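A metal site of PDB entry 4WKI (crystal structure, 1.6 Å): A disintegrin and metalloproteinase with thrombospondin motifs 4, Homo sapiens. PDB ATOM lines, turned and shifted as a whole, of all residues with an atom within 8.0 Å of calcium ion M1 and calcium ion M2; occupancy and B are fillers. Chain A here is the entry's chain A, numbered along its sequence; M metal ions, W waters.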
ATOM      1  N   PHE A   7       2.364 -11.066  -4.680  1.00  0.00           N
ATOM      2  CA  PHE A   7       1.641  -9.845  -5.054  1.00  0.00           C
ATOM      3  C   PHE A   7       2.508  -8.622  -4.781  1.00  0.00           C
ATOM      4  O   PHE A   7       2.958  -8.386  -3.657  1.00  0.00           O
ATOM      5  CB  PHE A   7       0.353  -9.722  -4.225  1.00  0.00           C
ATOM      6  CG  PHE A   7      -0.472 -10.973  -4.226  1.00  0.00           C
ATOM      7  CD1 PHE A   7      -0.289 -11.936  -3.233  1.00  0.00           C
ATOM      8  CD2 PHE A   7      -1.390 -11.209  -5.224  1.00  0.00           C
ATOM      9  CE1 PHE A   7      -1.030 -13.106  -3.238  1.00  0.00           C
ATOM     10  CE2 PHE A   7      -2.144 -12.378  -5.232  1.00  0.00           C
ATOM     11  CZ  PHE A   7      -1.954 -13.312  -4.237  1.00  0.00           C
ATOM     12  N   VAL A   8       2.721  -7.812  -5.812  1.00  0.00           N
ATOM     13  CA  VAL A   8       3.509  -6.593  -5.663  1.00  0.00           C
ATOM     14  C   VAL A   8       2.525  -5.447  -5.601  1.00  0.00           C
ATOM     15  O   VAL A   8       1.908  -5.093  -6.609  1.00  0.00           O
ATOM     16  CB  VAL A   8       4.459  -6.346  -6.844  1.00  0.00           C
ATOM     17  CG1 VAL A   8       5.354  -5.148  -6.569  1.00  0.00           C
ATOM     18  CG2 VAL A   8       5.291  -7.577  -7.162  1.00  0.00           C
ATOM     19  N   GLU A   9       2.341  -4.903  -4.399  1.00  0.00           N
ATOM     20  CA  GLU A   9       1.469  -3.760  -4.201  1.00  0.00           C
ATOM     21  C   GLU A   9       2.144  -2.493  -4.720  1.00  0.00           C
ATOM     22  O   GLU A   9       3.143  -2.014  -4.173  1.00  0.00           O
ATOM     23  CB  GLU A   9       1.082  -3.630  -2.732  1.00  0.00           C
ATOM     24  CG  GLU A   9       0.317  -4.836  -2.191  1.00  0.00           C
ATOM     25  CD  GLU A   9       0.157  -4.815  -0.683  1.00  0.00           C
ATOM     26  OE1 GLU A   9       1.174  -5.007   0.016  1.00  0.00           O
ATOM     27  OE2 GLU A   9      -0.938  -4.584  -0.153  1.00  0.00           O
ATOM     28  N   THR A  10       1.581  -1.946  -5.801  1.00  0.00           N
ATOM     29  CA  THR A  10       2.291  -0.949  -6.600  1.00  0.00           C
ATOM     30  C   THR A  10       1.681   0.443  -6.514  1.00  0.00           C
ATOM     31  O   THR A  10       0.499   0.647  -6.771  1.00  0.00           O
ATOM     32  CB  THR A  10       2.400  -1.394  -8.079  1.00  0.00           C
ATOM     33  OG1 THR A  10       2.939  -2.729  -8.165  1.00  0.00           O
ATOM     34  CG2 THR A  10       3.314  -0.436  -8.855  1.00  0.00           C
ATOM     35  N   THR A  55      -2.194  -0.567  -6.539  1.00  0.00           N
ATOM     36  CA  THR A  55      -2.970  -0.277  -5.302  1.00  0.00           C
ATOM     37  C   THR A  55      -3.145   1.228  -5.010  1.00  0.00           C
ATOM     38  O   THR A  55      -4.088   1.640  -4.300  1.00  0.00           O
ATOM     39  CB  THR A  55      -2.350  -0.980  -4.089  1.00  0.00           C
ATOM     40  OG1 THR A  55      -0.983  -0.556  -3.929  1.00  0.00           O
ATOM     41  CG2 THR A  55      -2.379  -2.477  -4.290  1.00  0.00           C
ATOM     42  N   THR A  89       3.832   3.813   4.366  1.00  0.00           N
ATOM     43  CA  THR A  89       3.652   3.599   5.801  1.00  0.00           C
ATOM     44  C   THR A  89       4.658   2.551   6.265  1.00  0.00           C
ATOM     45  O   THR A  89       5.182   1.782   5.458  1.00  0.00           O
ATOM     46  CB  THR A  89       2.216   3.160   6.102  1.00  0.00           C
ATOM     47  OG1 THR A  89       1.931   1.932   5.438  1.00  0.00           O
ATOM     48  CG2 THR A  89       1.229   4.243   5.651  1.00  0.00           C
ATOM     49  N   GLU A  91       4.481  -0.310   8.037  1.00  0.00           N
ATOM     50  CA  GLU A  91       4.137  -1.726   8.041  1.00  0.00           C
ATOM     51  C   GLU A  91       3.241  -2.125   6.868  1.00  0.00           C
ATOM     52  O   GLU A  91       2.298  -1.400   6.515  1.00  0.00           O
ATOM     53  CB  GLU A  91       3.455  -2.090   9.360  1.00  0.00           C
ATOM     54  CG  GLU A  91       4.249  -1.689  10.594  1.00  0.00           C
ATOM     55  CD  GLU A  91       5.603  -2.370  10.670  1.00  0.00           C
ATOM     56  OE1 GLU A  91       5.782  -3.439  10.035  1.00  0.00           O
ATOM     57  OE2 GLU A  91       6.492  -1.859  11.373  1.00  0.00           O
ATOM     58  N   ASP A  92       3.550  -3.297   6.316  1.00  0.00           N
ATOM     59  CA  ASP A  92       2.842  -3.859   5.155  1.00  0.00           C
ATOM     60  C   ASP A  92       1.390  -4.219   5.474  1.00  0.00           C
ATOM     61  O   ASP A  92       0.551  -4.310   4.564  1.00  0.00           O
ATOM     62  CB  ASP A  92       3.576  -5.082   4.613  1.00  0.00           C
ATOM     63  CG  ASP A  92       3.375  -5.279   3.128  1.00  0.00           C
ATOM     64  OD1 ASP A  92       2.516  -4.571   2.543  1.00  0.00           O
ATOM     65  OD2 ASP A  92       4.039  -6.156   2.564  1.00  0.00           O
ATOM     66  N   SER A  93       1.114  -4.421   6.766  1.00  0.00           N
ATOM     67  CA  SER A  93      -0.239  -4.609   7.306  1.00  0.00           C
ATOM     68  C   SER A  93      -1.209  -3.462   7.006  1.00  0.00           C
ATOM     69  O   SER A  93      -2.406  -3.678   6.922  1.00  0.00           O
ATOM     70  CB  SER A  93      -0.190  -4.797   8.846  1.00  0.00           C
ATOM     71  OG  SER A  93      -0.167  -3.532   9.519  1.00  0.00           O
ATOM     72  N   ASP A  94      -0.677  -2.247   6.884  1.00  0.00           N
ATOM     73  CA  ASP A  94      -1.475  -1.066   6.574  1.00  0.00           C
ATOM     74  C   ASP A  94      -1.917  -1.093   5.114  1.00  0.00           C
ATOM     75  O   ASP A  94      -1.082  -1.319   4.247  1.00  0.00           O
ATOM     76  CB  ASP A  94      -0.597   0.177   6.775  1.00  0.00           C
ATOM     77  CG  ASP A  94      -1.382   1.461   6.843  1.00  0.00           C
ATOM     78  OD1 ASP A  94      -1.072   2.279   7.735  1.00  0.00           O
ATOM     79  OD2 ASP A  94      -2.301   1.695   6.014  1.00  0.00           O
ATOM     80  N   PRO A  95      -3.220  -0.850   4.823  1.00  0.00           N
ATOM     81  CA  PRO A  95      -3.704  -0.832   3.423  1.00  0.00           C
ATOM     82  C   PRO A  95      -3.005   0.168   2.494  1.00  0.00           C
ATOM     83  O   PRO A  95      -2.939  -0.067   1.280  1.00  0.00           O
ATOM     84  CB  PRO A  95      -5.197  -0.474   3.541  1.00  0.00           C
ATOM     85  CG  PRO A  95      -5.571  -0.676   4.966  1.00  0.00           C
ATOM     86  CD  PRO A  95      -4.321  -0.761   5.807  1.00  0.00           C
ATOM     87  N   ASP A  96      -2.537   1.288   3.046  1.00  0.00           N
ATOM     88  CA  ASP A  96      -1.859   2.331   2.267  1.00  0.00           C
ATOM     89  C   ASP A  96      -0.425   1.945   1.940  1.00  0.00           C
ATOM     90  O   ASP A  96       0.221   2.605   1.113  1.00  0.00           O
ATOM     91  CB  ASP A  96      -1.836   3.654   3.038  1.00  0.00           C
ATOM     92  CG  ASP A  96      -3.192   4.307   3.113  1.00  0.00           C
ATOM     93  OD1 ASP A  96      -4.114   3.894   2.380  1.00  0.00           O
ATOM     94  OD2 ASP A  96      -3.328   5.259   3.910  1.00  0.00           O
ATOM     95  N   HIS A  97       0.100   0.918   2.592  1.00  0.00           N
ATOM     96  CA  HIS A  97       1.476   0.495   2.316  1.00  0.00           C
ATOM     97  C   HIS A  97       1.590  -0.075   0.915  1.00  0.00           C
ATOM     98  O   HIS A  97       0.703  -0.773   0.445  1.00  0.00           O
ATOM     99  CB  HIS A  97       1.969  -0.559   3.306  1.00  0.00           C
ATOM    100  CG  HIS A  97       3.418  -0.898   3.133  1.00  0.00           C
ATOM    101  ND1 HIS A  97       4.423  -0.184   3.751  1.00  0.00           N
ATOM    102  CD2 HIS A  97       4.031  -1.867   2.409  1.00  0.00           C
ATOM    103  CE1 HIS A  97       5.595  -0.695   3.405  1.00  0.00           C
ATOM    104  NE2 HIS A  97       5.386  -1.723   2.609  1.00  0.00           N
ATOM    105  N   PHE A  98       2.706   0.238   0.263  1.00  0.00           N
ATOM    106  CA  PHE A  98       3.003  -0.299  -1.048  1.00  0.00           C
ATOM    107  C   PHE A  98       4.420  -0.853  -1.093  1.00  0.00           C
ATOM    108  O   PHE A  98       5.307  -0.398  -0.324  1.00  0.00           O
ATOM    109  CB  PHE A  98       2.776   0.777  -2.144  1.00  0.00           C
ATOM    110  CG  PHE A  98       3.516   2.069  -1.906  1.00  0.00           C
ATOM    111  CD1 PHE A  98       4.812   2.218  -2.365  1.00  0.00           C
ATOM    112  CD2 PHE A  98       2.908   3.135  -1.245  1.00  0.00           C
ATOM    113  CE1 PHE A  98       5.500   3.407  -2.138  1.00  0.00           C
ATOM    114  CE2 PHE A  98       3.590   4.329  -1.024  1.00  0.00           C
ATOM    115  CZ  PHE A  98       4.898   4.460  -1.477  1.00  0.00           C
ATOM    116  N   ASP A  99       4.604  -1.829  -1.969  1.00  0.00           N
ATOM    117  CA  ASP A  99       5.844  -2.610  -2.100  1.00  0.00           C
ATOM    118  C   ASP A  99       6.833  -2.001  -3.115  1.00  0.00           C
ATOM    119  O   ASP A  99       8.028  -2.213  -3.001  1.00  0.00           O
ATOM    120  CB  ASP A  99       5.541  -4.065  -2.483  1.00  0.00           C
ATOM    121  CG  ASP A  99       4.664  -4.773  -1.463  1.00  0.00           C
ATOM    122  OD1 ASP A  99       4.874  -4.551  -0.250  1.00  0.00           O
ATOM    123  OD2 ASP A  99       3.783  -5.553  -1.881  1.00  0.00           O
ATOM    124  N   THR A 100       6.325  -1.305  -4.131  1.00  0.00           N
ATOM    125  CA  THR A 100       7.203  -0.673  -5.107  1.00  0.00           C
ATOM    126  C   THR A 100       6.539   0.586  -5.659  1.00  0.00           C
ATOM    127  O   THR A 100       5.311   0.741  -5.585  1.00  0.00           O
ATOM    128  CB  THR A 100       7.621  -1.660  -6.230  1.00  0.00           C
ATOM    129  OG1 THR A 100       8.836  -1.211  -6.851  1.00  0.00           O
ATOM    130  CG2 THR A 100       6.514  -1.814  -7.276  1.00  0.00           C
ATOM    131  N   VAL A 126      13.152  -4.882  -4.217  1.00  0.00           N
ATOM    132  CA  VAL A 126      11.683  -4.887  -4.196  1.00  0.00           C
ATOM    133  C   VAL A 126      11.051  -4.803  -2.803  1.00  0.00           C
ATOM    134  O   VAL A 126      10.017  -4.167  -2.645  1.00  0.00           O
ATOM    135  CB  VAL A 126      11.095  -6.095  -4.955  1.00  0.00           C
ATOM    136  CG1 VAL A 126      11.183  -7.370  -4.132  1.00  0.00           C
ATOM    137  CG2 VAL A 126       9.636  -5.843  -5.357  1.00  0.00           C
ATOM    138  N   CYS A 127      11.676  -5.422  -1.808  1.00  0.00           N
ATOM    139  CA  CYS A 127      11.127  -5.410  -0.441  1.00  0.00           C
ATOM    140  C   CYS A 127      11.817  -4.428   0.527  1.00  0.00           C
ATOM    141  O   CYS A 127      11.585  -4.437   1.755  1.00  0.00           O
ATOM    142  CB  CYS A 127      11.037  -6.841   0.104  1.00  0.00           C
ATOM    143  SG  CYS A 127       9.651  -7.688  -0.704  1.00  0.00           S
ATOM    144  N   GLY A 209      11.733 -11.517  -1.379  1.00  0.00           N
ATOM    145  CA  GLY A 209      10.354 -11.168  -1.703  1.00  0.00           C
ATOM    146  C   GLY A 209       9.390 -11.388  -0.551  1.00  0.00           C
ATOM    147  O   GLY A 209       8.203 -11.615  -0.762  1.00  0.00           O
ATOM    148  N   HIS A 210       9.898 -11.289   0.674  1.00  0.00           N
ATOM    149  CA  HIS A 210       9.115 -11.508   1.890  1.00  0.00           C
ATOM    150  C   HIS A 210       7.941 -10.538   2.079  1.00  0.00           C
ATOM    151  O   HIS A 210       6.994 -10.855   2.783  1.00  0.00           O
ATOM    152  CB  HIS A 210      10.054 -11.439   3.106  1.00  0.00           C
ATOM    153  CG  HIS A 210      10.737 -10.108   3.253  1.00  0.00           C
ATOM    154  ND1 HIS A 210      10.136  -9.026   3.859  1.00  0.00           N
ATOM    155  CD2 HIS A 210      11.963  -9.685   2.854  1.00  0.00           C
ATOM    156  CE1 HIS A 210      10.965  -8.000   3.837  1.00  0.00           C
ATOM    157  NE2 HIS A 210      12.074  -8.364   3.227  1.00  0.00           N
ATOM    158  N   CYS A 211       8.007  -9.367   1.442  1.00  0.00           N
ATOM    159  CA  CYS A 211       6.950  -8.362   1.510  1.00  0.00           C
ATOM    160  C   CYS A 211       5.881  -8.564   0.421  1.00  0.00           C
ATOM    161  O   CYS A 211       4.957  -7.774   0.330  1.00  0.00           O
ATOM    162  CB  CYS A 211       7.548  -6.971   1.387  1.00  0.00           C
ATOM    163  SG  CYS A 211       8.022  -6.521  -0.294  1.00  0.00           S
ATOM    164  N   LEU A 212       6.017  -9.605  -0.389  1.00  0.00           N
ATOM    165  CA  LEU A 212       5.108  -9.852  -1.515  1.00  0.00           C
ATOM    166  C   LEU A 212       4.077 -10.919  -1.175  1.00  0.00           C
ATOM    167  O   LEU A 212       3.397 -11.419  -2.054  1.00  0.00           O
ATOM    168  CB  LEU A 212       5.902 -10.254  -2.752  1.00  0.00           C
ATOM    169  CG  LEU A 212       7.008  -9.278  -3.172  1.00  0.00           C
ATOM    170  CD1 LEU A 212       7.796  -9.861  -4.322  1.00  0.00           C
ATOM    171  CD2 LEU A 212       6.428  -7.933  -3.550  1.00  0.00           C
ATOM    172  N   LEU A 213       3.952 -11.262   0.100  1.00  0.00           N
ATOM    173  CA  LEU A 213       3.145 -12.423   0.463  1.00  0.00           C
ATOM    174  C   LEU A 213       1.719 -12.103   0.868  1.00  0.00           C
ATOM    175  O   LEU A 213       0.856 -12.980   0.811  1.00  0.00           O
ATOM    176  CB  LEU A 213       3.858 -13.242   1.541  1.00  0.00           C
ATOM    177  CG  LEU A 213       5.146 -13.886   1.025  1.00  0.00           C
ATOM    178  CD1 LEU A 213       5.894 -14.542   2.165  1.00  0.00           C
ATOM    179  CD2 LEU A 213       4.839 -14.882  -0.087  1.00  0.00           C
ATOM    180  N   ASP A 214       1.471 -10.860   1.269  1.00  0.00           N
ATOM    181  CA  ASP A 214       0.133 -10.406   1.634  1.00  0.00           C
ATOM    182  C   ASP A 214      -0.671  -9.987   0.386  1.00  0.00           C
ATOM    183  O   ASP A 214      -0.125  -9.496  -0.593  1.00  0.00           O
ATOM    184  CB  ASP A 214       0.188  -9.289   2.690  1.00  0.00           C
ATOM    185  CG  ASP A 214       0.909  -8.031   2.217  1.00  0.00           C
ATOM    186  OD1 ASP A 214       1.992  -8.125   1.610  1.00  0.00           O
ATOM    187  OD2 ASP A 214       0.388  -6.939   2.523  1.00  0.00           O
ATOM    188  N   LYS A 215      -1.973 -10.232   0.434  1.00  0.00           N
ATOM    189  CA  LYS A 215      -2.813 -10.004  -0.724  1.00  0.00           C
ATOM    190  C   LYS A 215      -3.421  -8.621  -0.615  1.00  0.00           C
ATOM    191  O   LYS A 215      -3.971  -8.259   0.420  1.00  0.00           O
ATOM    192  CB  LYS A 215      -3.907 -11.085  -0.817  1.00  0.00           C
ATOM    193  CG  LYS A 215      -4.458 -11.277  -2.211  1.00  0.00           C
ATOM    194  CD  LYS A 215      -5.399 -12.469  -2.265  1.00  0.00           C
ATOM    195  CE  LYS A 215      -6.267 -12.454  -3.519  1.00  0.00           C
ATOM    196  NZ  LYS A 215      -5.689 -13.242  -4.644  1.00  0.00           N
ATOM    197  N   PRO A 216      -3.306  -7.816  -1.689  1.00  0.00           N
ATOM    198  CA  PRO A 216      -3.899  -6.488  -1.594  1.00  0.00           C
ATOM    199  C   PRO A 216      -5.422  -6.510  -1.414  1.00  0.00           C
ATOM    200  O   PRO A 216      -6.118  -7.382  -1.916  1.00  0.00           O
ATOM    201  CB  PRO A 216      -3.513  -5.812  -2.908  1.00  0.00           C
ATOM    202  CG  PRO A 216      -3.107  -6.895  -3.818  1.00  0.00           C
ATOM    203  CD  PRO A 216      -2.612  -8.036  -2.968  1.00  0.00           C
ATOM    204  N   GLU A 217      -5.880  -5.465  -0.744  1.00  0.00           N
ATOM    205  CA  GLU A 217      -7.247  -5.235  -0.325  1.00  0.00           C
ATOM    206  C   GLU A 217      -8.134  -4.796  -1.498  1.00  0.00           C
ATOM    207  O   GLU A 217      -9.160  -5.403  -1.830  1.00  0.00           O
ATOM    208  CB  GLU A 217      -7.173  -4.098   0.716  1.00  0.00           C
ATOM    209  CG  GLU A 217      -8.431  -3.784   1.509  1.00  0.00           C
ATOM    210  CD  GLU A 217      -8.201  -3.930   3.006  1.00  0.00           C
ATOM    211  OE1 GLU A 217      -8.286  -2.910   3.722  1.00  0.00           O
ATOM    212  OE2 GLU A 217      -7.921  -5.060   3.453  1.00  0.00           O
HETATM  213 CA    CA M   1       3.104  -6.300   0.360  1.00  0.00          CA
HETATM  214 CA    CA M   2       0.082  -4.824   2.154  1.00  0.00          CA
HETATM  215  O   HOH W   1       2.049  -7.824  -1.228  1.00  0.00           O
HETATM  216  O   HOH W   2      -2.164  -5.427   2.679  1.00  0.00           O
HETATM  217  O   HOH W   3      -0.547  -2.614   1.962  1.00  0.00           O
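SG of Cys 127 forms a disulfide with SG of Cys 211 (2.0 Å). The backbone carbonyl oxygen (O) of Glu 9 is in hydrogen-bond range of the backbone NH (N) of Thr 100 (3.3 Å).
Five residues have an atom within 4 Å of calcium ion M1: Glu 9, Asp 92, Asp 99, Cys 211 and Asp 214. Along chain A the residues within 4 Å of calcium ion M1 span positions 9 to 214.
Three residues have an atom within 4 Å of calcium ion M2: Glu 9, Asp 92 and Asp 214. The nearest printed residue that does not touch calcium ion M2 is Asp 94 (4.2 Å).
Calcium ion M1 is bound by OE1 of Glu 9 (2.3 Å), O of Cys 211 (2.4 Å), OD2 of Asp 92 (2.4 Å), water W1 (2.4 Å), OD2 of Asp 99 (2.5 Å), OD1 of Asp 214 (2.5 Å), OD1 of Asp 99 (2.6 Å) and OD1 of Asp 92 (2.8 Å).
Calcium ion M2 is bound by the side-chain carboxylate (OD2) of Asp 214 (2.2 Å), water W3 (2.3 Å), water W2 (2.4 Å), the side-chain carboxylate (OE1) of Glu 9 (2.4 Å), the side-chain carboxylate (OD1) of Asp 92 (2.5 Å), the backbone carbonyl oxygen (O) of Asp 92 (2.5 Å) and the side-chain carboxylate (OE2) of Glu 9 (2.5 Å). Calcium ion M2 has seven donor atoms within binding distance.
Water W1 lies within hydrogen-bond range of the backbone carbonyl oxygen (O) of Phe 7 (2.7 Å) and the backbone carbonyl oxygen (O) of Asp 214 (2.8 Å).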
